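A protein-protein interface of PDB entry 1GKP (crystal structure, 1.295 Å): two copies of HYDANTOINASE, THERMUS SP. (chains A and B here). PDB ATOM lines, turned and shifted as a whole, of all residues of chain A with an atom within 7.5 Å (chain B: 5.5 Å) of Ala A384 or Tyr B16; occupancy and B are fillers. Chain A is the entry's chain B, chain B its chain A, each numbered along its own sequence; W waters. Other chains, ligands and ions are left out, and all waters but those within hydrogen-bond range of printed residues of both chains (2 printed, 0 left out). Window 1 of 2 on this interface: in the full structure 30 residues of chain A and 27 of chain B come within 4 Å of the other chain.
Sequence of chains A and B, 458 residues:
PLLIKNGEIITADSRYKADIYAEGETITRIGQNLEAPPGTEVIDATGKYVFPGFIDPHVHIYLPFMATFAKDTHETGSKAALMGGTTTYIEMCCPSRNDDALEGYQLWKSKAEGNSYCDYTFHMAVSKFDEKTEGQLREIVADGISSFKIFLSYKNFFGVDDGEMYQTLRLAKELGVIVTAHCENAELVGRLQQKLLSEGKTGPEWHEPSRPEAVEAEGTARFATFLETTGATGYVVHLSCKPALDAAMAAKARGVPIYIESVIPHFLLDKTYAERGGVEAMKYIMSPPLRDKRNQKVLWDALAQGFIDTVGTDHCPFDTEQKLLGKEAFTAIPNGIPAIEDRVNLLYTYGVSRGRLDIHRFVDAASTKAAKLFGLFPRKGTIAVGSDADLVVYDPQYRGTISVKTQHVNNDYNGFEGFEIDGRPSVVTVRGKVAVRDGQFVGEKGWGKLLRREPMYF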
ATOM      1  N   ILE A   9     -23.089   5.950   1.219  1.00  0.00           N
ATOM      2  CA  ILE A   9     -23.414   5.263   2.465  1.00  0.00           C
ATOM      3  C   ILE A   9     -24.825   5.612   2.838  1.00  0.00           C
ATOM      4  O   ILE A   9     -25.167   6.778   2.955  1.00  0.00           O
ATOM      5  CB  ILE A   9     -22.397   5.623   3.525  1.00  0.00           C
ATOM      6  CG1 ILE A   9     -20.941   5.199   3.094  1.00  0.00           C
ATOM      7  CG2 ILE A   9     -22.815   4.960   4.813  1.00  0.00           C
ATOM      8  CD1 ILE A   9     -19.808   5.904   3.810  1.00  0.00           C
ATOM      9  N   THR A  11     -27.719   4.561   5.753  1.00  0.00           N
ATOM     10  CA  THR A  11     -28.194   3.870   6.959  1.00  0.00           C
ATOM     11  C   THR A  11     -29.606   4.310   7.220  1.00  0.00           C
ATOM     12  O   THR A  11     -30.172   5.110   6.493  1.00  0.00           O
ATOM     13  CB  THR A  11     -27.298   4.111   8.189  1.00  0.00           C
ATOM     14  OG1 THR A  11     -27.459   5.447   8.629  1.00  0.00           O
ATOM     15  CG2 THR A  11     -25.840   3.878   7.916  1.00  0.00           C
ATOM     16  N   TYR A  16     -24.717   9.673   2.844  1.00  0.00           N
ATOM     17  CA  TYR A  16     -23.597  10.568   2.535  1.00  0.00           C
ATOM     18  C   TYR A  16     -22.577   9.811   1.723  1.00  0.00           C
ATOM     19  O   TYR A  16     -22.517   8.596   1.761  1.00  0.00           O
ATOM     20  CB  TYR A  16     -23.020  11.036   3.859  1.00  0.00           C
ATOM     21  CG  TYR A  16     -22.497   9.978   4.778  1.00  0.00           C
ATOM     22  CD1 TYR A  16     -23.388   9.203   5.540  1.00  0.00           C
ATOM     23  CD2 TYR A  16     -21.134   9.715   4.894  1.00  0.00           C
ATOM     24  CE1 TYR A  16     -22.929   8.250   6.385  1.00  0.00           C
ATOM     25  CE2 TYR A  16     -20.670   8.736   5.719  1.00  0.00           C
ATOM     26  CZ  TYR A  16     -21.546   8.023   6.484  1.00  0.00           C
ATOM     27  OH  TYR A  16     -21.121   7.005   7.316  1.00  0.00           O
ATOM     28  N   ILE A  20     -15.028   4.209   4.050  1.00  0.00           N
ATOM     29  CA  ILE A  20     -15.021   3.443   5.294  1.00  0.00           C
ATOM     30  C   ILE A  20     -13.767   2.581   5.312  1.00  0.00           C
ATOM     31  O   ILE A  20     -13.536   1.818   4.391  1.00  0.00           O
ATOM     32  CB  ILE A  20     -16.231   2.489   5.321  1.00  0.00           C
ATOM     33  CG1 ILE A  20     -17.533   3.278   5.290  1.00  0.00           C
ATOM     34  CG2 ILE A  20     -16.215   1.611   6.565  1.00  0.00           C
ATOM     35  CD1 ILE A  20     -18.710   2.434   4.947  1.00  0.00           C
ATOM     36  N   THR A  26     -13.726  -4.477  12.836  1.00  0.00           N
ATOM     37  CA  THR A  26     -14.611  -3.385  13.096  1.00  0.00           C
ATOM     38  C   THR A  26     -14.243  -2.121  12.318  1.00  0.00           C
ATOM     39  O   THR A  26     -13.086  -1.937  11.898  1.00  0.00           O
ATOM     40  CB  THR A  26     -14.696  -3.091  14.605  1.00  0.00           C
ATOM     41  OG1 THR A  26     -13.391  -2.765  15.087  1.00  0.00           O
ATOM     42  CG2 THR A  26     -15.204  -4.294  15.434  1.00  0.00           C
ATOM     43  N   ILE A  27     -15.213  -1.255  12.077  1.00  0.00           N
ATOM     44  CA  ILE A  27     -15.012   0.050  11.422  1.00  0.00           C
ATOM     45  C   ILE A  27     -14.112   0.895  12.305  1.00  0.00           C
ATOM     46  O   ILE A  27     -14.385   1.091  13.463  1.00  0.00           O
ATOM     47  CB  ILE A  27     -16.345   0.758  11.103  1.00  0.00           C
ATOM     48  CG1 ILE A  27     -17.145  -0.129  10.153  1.00  0.00           C
ATOM     49  CG2 ILE A  27     -16.061   2.080  10.484  1.00  0.00           C
ATOM     50  CD1 ILE A  27     -18.508   0.445   9.617  1.00  0.00           C
ATOM     51  N   THR A  28     -13.070   1.413  11.682  1.00  0.00           N
ATOM     52  CA  THR A  28     -12.007   2.135  12.351  1.00  0.00           C
ATOM     53  C   THR A  28     -12.169   3.622  12.136  1.00  0.00           C
ATOM     54  O   THR A  28     -12.020   4.409  13.050  1.00  0.00           O
ATOM     55  CB  THR A  28     -10.628   1.628  11.746  1.00  0.00           C
ATOM     56  OG1 THR A  28     -10.447   0.237  12.020  1.00  0.00           O
ATOM     57  CG2 THR A  28      -9.433   2.364  12.304  1.00  0.00           C
ATOM     58  N   ARG A  29     -12.403   4.010  10.880  1.00  0.00           N
ATOM     59  CA  ARG A  29     -12.587   5.408  10.560  1.00  0.00           C
ATOM     60  C   ARG A  29     -13.480   5.600   9.347  1.00  0.00           C
ATOM     61  O   ARG A  29     -13.533   4.758   8.489  1.00  0.00           O
ATOM     62  CB  ARG A  29     -11.233   6.152  10.336  1.00  0.00           C
ATOM     63  CG  ARG A  29     -10.163   5.451   9.601  1.00  0.00           C
ATOM     64  CD  ARG A  29      -8.899   6.337   9.339  1.00  0.00           C
ATOM     65  NE  ARG A  29      -7.745   5.497   9.033  1.00  0.00           N
ATOM     66  CZ  ARG A  29      -6.847   5.150   9.930  1.00  0.00           C
ATOM     67  NH1 ARG A  29      -6.949   5.616  11.169  1.00  0.00           N
ATOM     68  NH2 ARG A  29      -5.836   4.356   9.600  1.00  0.00           N
ATOM     69  N   ILE A  30     -14.197   6.716   9.337  1.00  0.00           N
ATOM     70  CA  ILE A  30     -15.042   7.143   8.198  1.00  0.00           C
ATOM     71  C   ILE A  30     -14.645   8.565   7.822  1.00  0.00           C
ATOM     72  O   ILE A  30     -14.482   9.411   8.685  1.00  0.00           O
ATOM     73  CB  ILE A  30     -16.546   7.022   8.526  1.00  0.00           C
ATOM     74  CG1 ILE A  30     -16.885   5.575   8.897  1.00  0.00           C
ATOM     75  CG2 ILE A  30     -17.342   7.463   7.302  1.00  0.00           C
ATOM     76  CD1 ILE A  30     -18.346   5.334   9.408  1.00  0.00           C
ATOM     77  N   PHE A 377     -27.262  -4.937  18.410  1.00  0.00           N
ATOM     78  CA  PHE A 377     -26.902  -3.557  18.135  1.00  0.00           C
ATOM     79  C   PHE A 377     -26.067  -3.068  19.307  1.00  0.00           C
ATOM     80  O   PHE A 377     -26.424  -3.390  20.416  1.00  0.00           O
ATOM     81  CB  PHE A 377     -28.211  -2.731  18.087  1.00  0.00           C
ATOM     82  CG  PHE A 377     -28.055  -1.247  17.884  1.00  0.00           C
ATOM     83  CD1 PHE A 377     -27.918  -0.404  18.963  1.00  0.00           C
ATOM     84  CD2 PHE A 377     -28.029  -0.680  16.606  1.00  0.00           C
ATOM     85  CE1 PHE A 377     -27.804   0.974  18.794  1.00  0.00           C
ATOM     86  CE2 PHE A 377     -27.888   0.678  16.440  1.00  0.00           C
ATOM     87  CZ  PHE A 377     -27.743   1.500  17.520  1.00  0.00           C
ATOM     88  N   PRO A 378     -25.065  -2.212  19.105  1.00  0.00           N
ATOM     89  CA  PRO A 378     -24.584  -1.694  17.827  1.00  0.00           C
ATOM     90  C   PRO A 378     -23.515  -2.522  17.144  1.00  0.00           C
ATOM     91  O   PRO A 378     -23.010  -2.041  16.118  1.00  0.00           O
ATOM     92  CB  PRO A 378     -24.034  -0.328  18.203  1.00  0.00           C
ATOM     93  CG  PRO A 378     -23.655  -0.445  19.623  1.00  0.00           C
ATOM     94  CD  PRO A 378     -24.372  -1.569  20.236  1.00  0.00           C
ATOM     95  N   ARG A 379     -23.174  -3.713  17.589  1.00  0.00           N
ATOM     96  CA  ARG A 379     -22.226  -4.554  16.894  1.00  0.00           C
ATOM     97  C   ARG A 379     -22.724  -4.709  15.441  1.00  0.00           C
ATOM     98  O   ARG A 379     -21.942  -4.664  14.508  1.00  0.00           O
ATOM     99  CB  ARG A 379     -22.100  -5.972  17.508  1.00  0.00           C
ATOM    100  CG  ARG A 379     -21.378  -6.132  18.799  1.00  0.00           C
ATOM    101  CD  ARG A 379     -21.427  -7.596  19.257  1.00  0.00           C
ATOM    102  NE  ARG A 379     -22.730  -7.884  19.830  1.00  0.00           N
ATOM    103  CZ  ARG A 379     -23.137  -9.015  20.397  1.00  0.00           C
ATOM    104  NH1 ARG A 379     -22.402 -10.113  20.419  1.00  0.00           N
ATOM    105  NH2 ARG A 379     -24.365  -9.009  20.890  1.00  0.00           N
ATOM    106  N   GLY A 381     -26.109  -4.051  12.515  1.00  0.00           N
ATOM    107  CA  GLY A 381     -27.264  -3.235  12.182  1.00  0.00           C
ATOM    108  C   GLY A 381     -27.011  -1.837  11.766  1.00  0.00           C
ATOM    109  O   GLY A 381     -27.910  -1.099  11.407  1.00  0.00           O
ATOM    110  N   THR A 382     -25.756  -1.424  11.789  1.00  0.00           N
ATOM    111  CA  THR A 382     -25.538  -0.044  11.382  1.00  0.00           C
ATOM    112  C   THR A 382     -24.143   0.170  10.802  1.00  0.00           C
ATOM    113  O   THR A 382     -23.347  -0.753  10.706  1.00  0.00           O
ATOM    114  CB  THR A 382     -25.902   0.963  12.476  1.00  0.00           C
ATOM    115  OG1 THR A 382     -26.189   2.293  11.924  1.00  0.00           O
ATOM    116  CG2 THR A 382     -24.819   1.133  13.478  1.00  0.00           C
ATOM    117  N   ILE A 383     -23.874   1.388  10.384  1.00  0.00           N
ATOM    118  CA  ILE A 383     -22.535   1.768   9.924  1.00  0.00           C
ATOM    119  C   ILE A 383     -22.105   2.903  10.805  1.00  0.00           C
ATOM    120  O   ILE A 383     -22.629   3.985  10.701  1.00  0.00           O
ATOM    121  CB  ILE A 383     -22.543   2.185   8.414  1.00  0.00           C
ATOM    122  CG1 ILE A 383     -22.873   0.977   7.539  1.00  0.00           C
ATOM    123  CG2 ILE A 383     -21.177   2.763   8.035  1.00  0.00           C
ATOM    124  CD1 ILE A 383     -23.033   1.272   6.000  1.00  0.00           C
ATOM    125  N   ALA A 384     -21.114   2.645  11.648  1.00  0.00           N
ATOM    126  CA  ALA A 384     -20.549   3.631  12.534  1.00  0.00           C
ATOM    127  C   ALA A 384     -19.230   3.090  12.993  1.00  0.00           C
ATOM    128  O   ALA A 384     -19.026   1.917  13.106  1.00  0.00           O
ATOM    129  CB  ALA A 384     -21.420   3.832  13.729  1.00  0.00           C
ATOM    130  N   VAL A 385     -18.313   3.994  13.290  1.00  0.00           N
ATOM    131  CA  VAL A 385     -17.067   3.545  13.926  1.00  0.00           C
ATOM    132  C   VAL A 385     -17.329   2.634  15.125  1.00  0.00           C
ATOM    133  O   VAL A 385     -18.245   2.888  15.927  1.00  0.00           O
ATOM    134  CB  VAL A 385     -16.267   4.741  14.348  1.00  0.00           C
ATOM    135  CG1 VAL A 385     -15.021   4.300  15.134  1.00  0.00           C
ATOM    136  CG2 VAL A 385     -15.823   5.577  13.143  1.00  0.00           C
ATOM    137  N   GLY A 386     -16.600   1.529  15.187  1.00  0.00           N
ATOM    138  CA  GLY A 386     -16.753   0.591  16.301  1.00  0.00           C
ATOM    139  C   GLY A 386     -17.641  -0.599  15.999  1.00  0.00           C
ATOM    140  O   GLY A 386     -17.583  -1.646  16.635  1.00  0.00           O
ATOM    141  N   SER A 387     -18.449  -0.467  14.965  1.00  0.00           N
ATOM    142  CA  SER A 387     -19.371  -1.512  14.596  1.00  0.00           C
ATOM    143  C   SER A 387     -18.699  -2.599  13.772  1.00  0.00           C
ATOM    144  O   SER A 387     -17.646  -2.358  13.207  1.00  0.00           O
ATOM    145  CB  SER A 387     -20.594  -0.884  13.957  1.00  0.00           C
ATOM    146  OG  SER A 387     -21.376  -0.148  14.918  1.00  0.00           O
ATOM    147  N   ASP A 388     -19.152  -3.822  13.829  1.00  0.00           N
ATOM    148  CA  ASP A 388     -18.601  -4.862  13.027  1.00  0.00           C
ATOM    149  C   ASP A 388     -18.686  -4.426  11.584  1.00  0.00           C
ATOM    150  O   ASP A 388     -19.689  -3.825  11.126  1.00  0.00           O
ATOM    151  CB  ASP A 388     -19.354  -6.191  13.227  1.00  0.00           C
ATOM    152  CG  ASP A 388     -19.144  -6.821  14.592  1.00  0.00           C
ATOM    153  OD1 ASP A 388     -18.326  -6.329  15.392  1.00  0.00           O
ATOM    154  OD2 ASP A 388     -19.706  -7.913  14.759  1.00  0.00           O
ATOM    155  N   ALA A 389     -17.633  -4.711  10.849  1.00  0.00           N
ATOM    156  CA  ALA A 389     -17.539  -4.291   9.476  1.00  0.00           C
ATOM    157  C   ALA A 389     -18.226  -5.274   8.567  1.00  0.00           C
ATOM    158  O   ALA A 389     -17.655  -6.029   7.807  1.00  0.00           O
ATOM    159  CB  ALA A 389     -16.078  -4.059   9.113  1.00  0.00           C
ATOM    160  N   LEU A 391     -20.804  -5.207   5.859  1.00  0.00           N
ATOM    161  CA  LEU A 391     -21.183  -4.173   4.894  1.00  0.00           C
ATOM    162  C   LEU A 391     -21.635  -4.800   3.586  1.00  0.00           C
ATOM    163  O   LEU A 391     -21.159  -5.863   3.150  1.00  0.00           O
ATOM    164  CB  LEU A 391     -19.969  -3.277   4.649  1.00  0.00           C
ATOM    165  CG  LEU A 391     -19.540  -2.486   5.872  1.00  0.00           C
ATOM    166  CD1 LEU A 391     -18.088  -1.953   5.639  1.00  0.00           C
ATOM    167  CD2 LEU A 391     -20.414  -1.394   6.329  1.00  0.00           C
ATOM    168  N   GLY B   7     -16.498  11.611  23.668  1.00  0.00           N
ATOM    169  CA  GLY B   7     -17.932  11.467  23.865  1.00  0.00           C
ATOM    170  C   GLY B   7     -18.507  10.169  23.377  1.00  0.00           C
ATOM    171  O   GLY B   7     -17.874   9.377  22.688  1.00  0.00           O
ATOM    172  N   GLU B   8     -19.715   9.917  23.868  1.00  0.00           N
ATOM    173  CA  GLU B   8     -20.514   8.795  23.382  1.00  0.00           C
ATOM    174  C   GLU B   8     -21.528   9.410  22.384  1.00  0.00           C
ATOM    175  O   GLU B   8     -22.470  10.105  22.742  1.00  0.00           O
ATOM    176  CB  GLU B   8     -21.201   8.016  24.495  1.00  0.00           C
ATOM    177  CG  GLU B   8     -21.899   6.788  23.951  1.00  0.00           C
ATOM    178  CD  GLU B   8     -22.682   6.006  24.981  1.00  0.00           C
ATOM    179  OE1 GLU B   8     -23.151   6.587  25.972  1.00  0.00           O
ATOM    180  OE2 GLU B   8     -22.821   4.794  24.771  1.00  0.00           O
ATOM    181  N   ILE B   9     -21.286   9.117  21.116  1.00  0.00           N
ATOM    182  CA  ILE B   9     -22.100   9.597  20.002  1.00  0.00           C
ATOM    183  C   ILE B   9     -23.406   8.784  19.927  1.00  0.00           C
ATOM    184  O   ILE B   9     -23.363   7.557  19.935  1.00  0.00           O
ATOM    185  CB  ILE B   9     -21.303   9.496  18.699  1.00  0.00           C
ATOM    186  CG1 ILE B   9     -20.051  10.410  18.770  1.00  0.00           C
ATOM    187  CG2 ILE B   9     -22.164   9.908  17.553  1.00  0.00           C
ATOM    188  CD1 ILE B   9     -19.106  10.192  17.662  1.00  0.00           C
ATOM    189  N   ILE B  10     -24.529   9.471  19.965  1.00  0.00           N
ATOM    190  CA  ILE B  10     -25.831   8.823  19.904  1.00  0.00           C
ATOM    191  C   ILE B  10     -26.698   9.479  18.852  1.00  0.00           C
ATOM    192  O   ILE B  10     -27.029  10.651  18.915  1.00  0.00           O
ATOM    193  CB  ILE B  10     -26.539   8.808  21.274  1.00  0.00           C
ATOM    194  CG1 ILE B  10     -25.617   8.223  22.388  1.00  0.00           C
ATOM    195  CG2 ILE B  10     -27.821   8.040  21.168  1.00  0.00           C
ATOM    196  CD1 ILE B  10     -26.242   8.242  23.796  1.00  0.00           C
ATOM    197  N   SER B  14     -27.331   4.805  15.842  1.00  0.00           N
ATOM    198  CA  SER B  14     -25.943   4.519  16.213  1.00  0.00           C
ATOM    199  C   SER B  14     -25.689   4.951  17.647  1.00  0.00           C
ATOM    200  O   SER B  14     -26.393   5.805  18.129  1.00  0.00           O
ATOM    201  CB  SER B  14     -24.976   5.214  15.224  1.00  0.00           C
ATOM    202  OG  SER B  14     -24.935   6.630  15.375  1.00  0.00           O
ATOM    203  N   ARG B  15     -24.758   4.267  18.331  1.00  0.00           N
ATOM    204  CA  ARG B  15     -24.360   4.591  19.698  1.00  0.00           C
ATOM    205  C   ARG B  15     -22.960   4.040  19.871  1.00  0.00           C
ATOM    206  O   ARG B  15     -22.810   2.840  19.934  1.00  0.00           O
ATOM    207  CB  ARG B  15     -25.307   3.958  20.693  1.00  0.00           C
ATOM    208  CG  ARG B  15     -24.913   4.266  22.105  1.00  0.00           C
ATOM    209  CD  ARG B  15     -25.982   3.981  23.141  1.00  0.00           C
ATOM    210  NE  ARG B  15     -25.621   4.531  24.427  1.00  0.00           N
ATOM    211  CZ  ARG B  15     -26.457   4.800  25.401  1.00  0.00           C
ATOM    212  NH1 ARG B  15     -27.749   4.543  25.282  1.00  0.00           N
ATOM    213  NH2 ARG B  15     -25.999   5.388  26.493  1.00  0.00           N
ATOM    214  N   TYR B  16     -21.931   4.892  19.954  1.00  0.00           N
ATOM    215  CA  TYR B  16     -20.544   4.467  19.975  1.00  0.00           C
ATOM    216  C   TYR B  16     -19.664   5.578  20.483  1.00  0.00           C
ATOM    217  O   TYR B  16     -20.039   6.736  20.455  1.00  0.00           O
ATOM    218  CB  TYR B  16     -20.106   4.107  18.596  1.00  0.00           C
ATOM    219  CG  TYR B  16     -20.217   5.229  17.602  1.00  0.00           C
ATOM    220  CD1 TYR B  16     -21.449   5.635  17.053  1.00  0.00           C
ATOM    221  CD2 TYR B  16     -19.065   5.904  17.166  1.00  0.00           C
ATOM    222  CE1 TYR B  16     -21.523   6.699  16.127  1.00  0.00           C
ATOM    223  CE2 TYR B  16     -19.142   6.941  16.251  1.00  0.00           C
ATOM    224  CZ  TYR B  16     -20.346   7.333  15.724  1.00  0.00           C
ATOM    225  OH  TYR B  16     -20.439   8.346  14.785  1.00  0.00           O
ATOM    226  N   LYS B  17     -18.490   5.195  20.981  1.00  0.00           N
ATOM    227  CA  LYS B  17     -17.529   6.157  21.513  1.00  0.00           C
ATOM    228  C   LYS B  17     -16.469   6.408  20.482  1.00  0.00           C
ATOM    229  O   LYS B  17     -15.752   5.518  20.091  1.00  0.00           O
ATOM    230  CB  LYS B  17     -16.938   5.605  22.785  1.00  0.00           C
ATOM    231  CG  LYS B  17     -17.933   5.693  23.943  1.00  0.00           C
ATOM    232  CD  LYS B  17     -17.471   5.057  25.234  1.00  0.00           C
ATOM    233  CE  LYS B  17     -18.462   5.371  26.354  1.00  0.00           C
ATOM    234  NZ  LYS B  17     -18.064   4.812  27.687  1.00  0.00           N
ATOM    235  N   ALA B  18     -16.439   7.630  19.983  1.00  0.00           N
ATOM    236  CA  ALA B  18     -15.424   8.024  19.005  1.00  0.00           C
ATOM    237  C   ALA B  18     -15.327   9.523  18.990  1.00  0.00           C
ATOM    238  O   ALA B  18     -16.060  10.172  19.689  1.00  0.00           O
ATOM    239  CB  ALA B  18     -15.766   7.530  17.629  1.00  0.00           C
ATOM    240  N   ILE B  30     -14.625  10.866  11.383  1.00  0.00           N
ATOM    241  CA  ILE B  30     -15.009  10.305  12.682  1.00  0.00           C
ATOM    242  C   ILE B  30     -14.114   9.102  12.912  1.00  0.00           C
ATOM    243  O   ILE B  30     -13.922   8.281  12.042  1.00  0.00           O
ATOM    244  CB  ILE B  30     -16.530   9.905  12.679  1.00  0.00           C
ATOM    245  CG1 ILE B  30     -17.404  11.118  12.388  1.00  0.00           C
ATOM    246  CG2 ILE B  30     -16.934   9.295  13.994  1.00  0.00           C
ATOM    247  CD1 ILE B  30     -18.933  10.755  12.232  1.00  0.00           C
ATOM    248  N   ILE B 383     -25.599  12.669  12.594  1.00  0.00           N
ATOM    249  CA  ILE B 383     -24.168  12.804  12.764  1.00  0.00           C
ATOM    250  C   ILE B 383     -23.563  11.835  11.780  1.00  0.00           C
ATOM    251  O   ILE B 383     -23.639  10.621  11.944  1.00  0.00           O
ATOM    252  CB  ILE B 383     -23.707  12.501  14.221  1.00  0.00           C
ATOM    253  CG1 ILE B 383     -24.255  13.555  15.161  1.00  0.00           C
ATOM    254  CG2 ILE B 383     -22.167  12.535  14.314  1.00  0.00           C
ATOM    255  CD1 ILE B 383     -23.953  13.268  16.675  1.00  0.00           C
HETATM  256  O   HOH W   1     -16.046   3.278  18.480  1.00  0.00           O
HETATM  257  O   HOH W   2     -19.121   6.751  12.760  1.00  0.00           O
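N of Ile B30 sits at hydrogen-bond distance from O of Ile A30, 3.1 Å away.
The side-chain carboxylate (OE2) of Glu B8 lies within salt-bridge range of the guanidinium group (NE) of Arg B15, 2.8 Å away. The backbone carbonyl oxygen of Tyr B16 is in hydrogen-bond range of the backbone NH of Ile B9 (2.8 Å). OG of Ser A387 sits at hydrogen-bond distance from O of Pro A378, 2.8 Å away.
Among the printed residues, merely in contact across the chains: Arg A29 with Ile B30 (3.5 Å), Phe A377 with Ser B14 (3.7 Å), Pro A378 with Arg B15 (3.4 Å), Ala A384 with Tyr B16 (3.7 Å), Val A385 with Tyr B16 (3.4 Å) and Val A385 with Ile B30 (3.5 Å).
Ala A384 touches one residue of chain B. Printed residues of chain A within 4 Å of Ile B30: Arg A29 (3.5 Å), Ile A30 (3.1 Å) and Val A385 (3.5 Å). Of the printed residues of chain B, Arg A29 touches Ile B30 (3.5 Å).
Printed residues of chain A that touch a printed residue of chain B: Arg A29, Ile A30, Phe A377, Pro A378, Ala A384 and Val A385. Hydrophobic or aromatic side chains of chain A that line the printed part of chain B: Phe A377, Pro A378, Ala A384 and Val A385. Among the printed residues, 7 pairs touch across the chains. Among the printed residues, no Asp or Glu carboxylate lies within 4 Å of a Lys or Arg side-chain nitrogen of the other chain.
Ile A30 touches its own counterpart, Ile B30. Of the 7 pairs that touch across the chains among the printed residues, 1 has its exchanged pair printed and touching as well.
Water W1 lies within hydrogen-bond range of O of Lys B17 (2.8 Å) and O of Val A385 (3.4 Å). Water W2 bridges the side-chain hydroxyl (OH) of Tyr B16 (2.9 Å) and the backbone NH (N) of Val A385 (2.9 Å).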
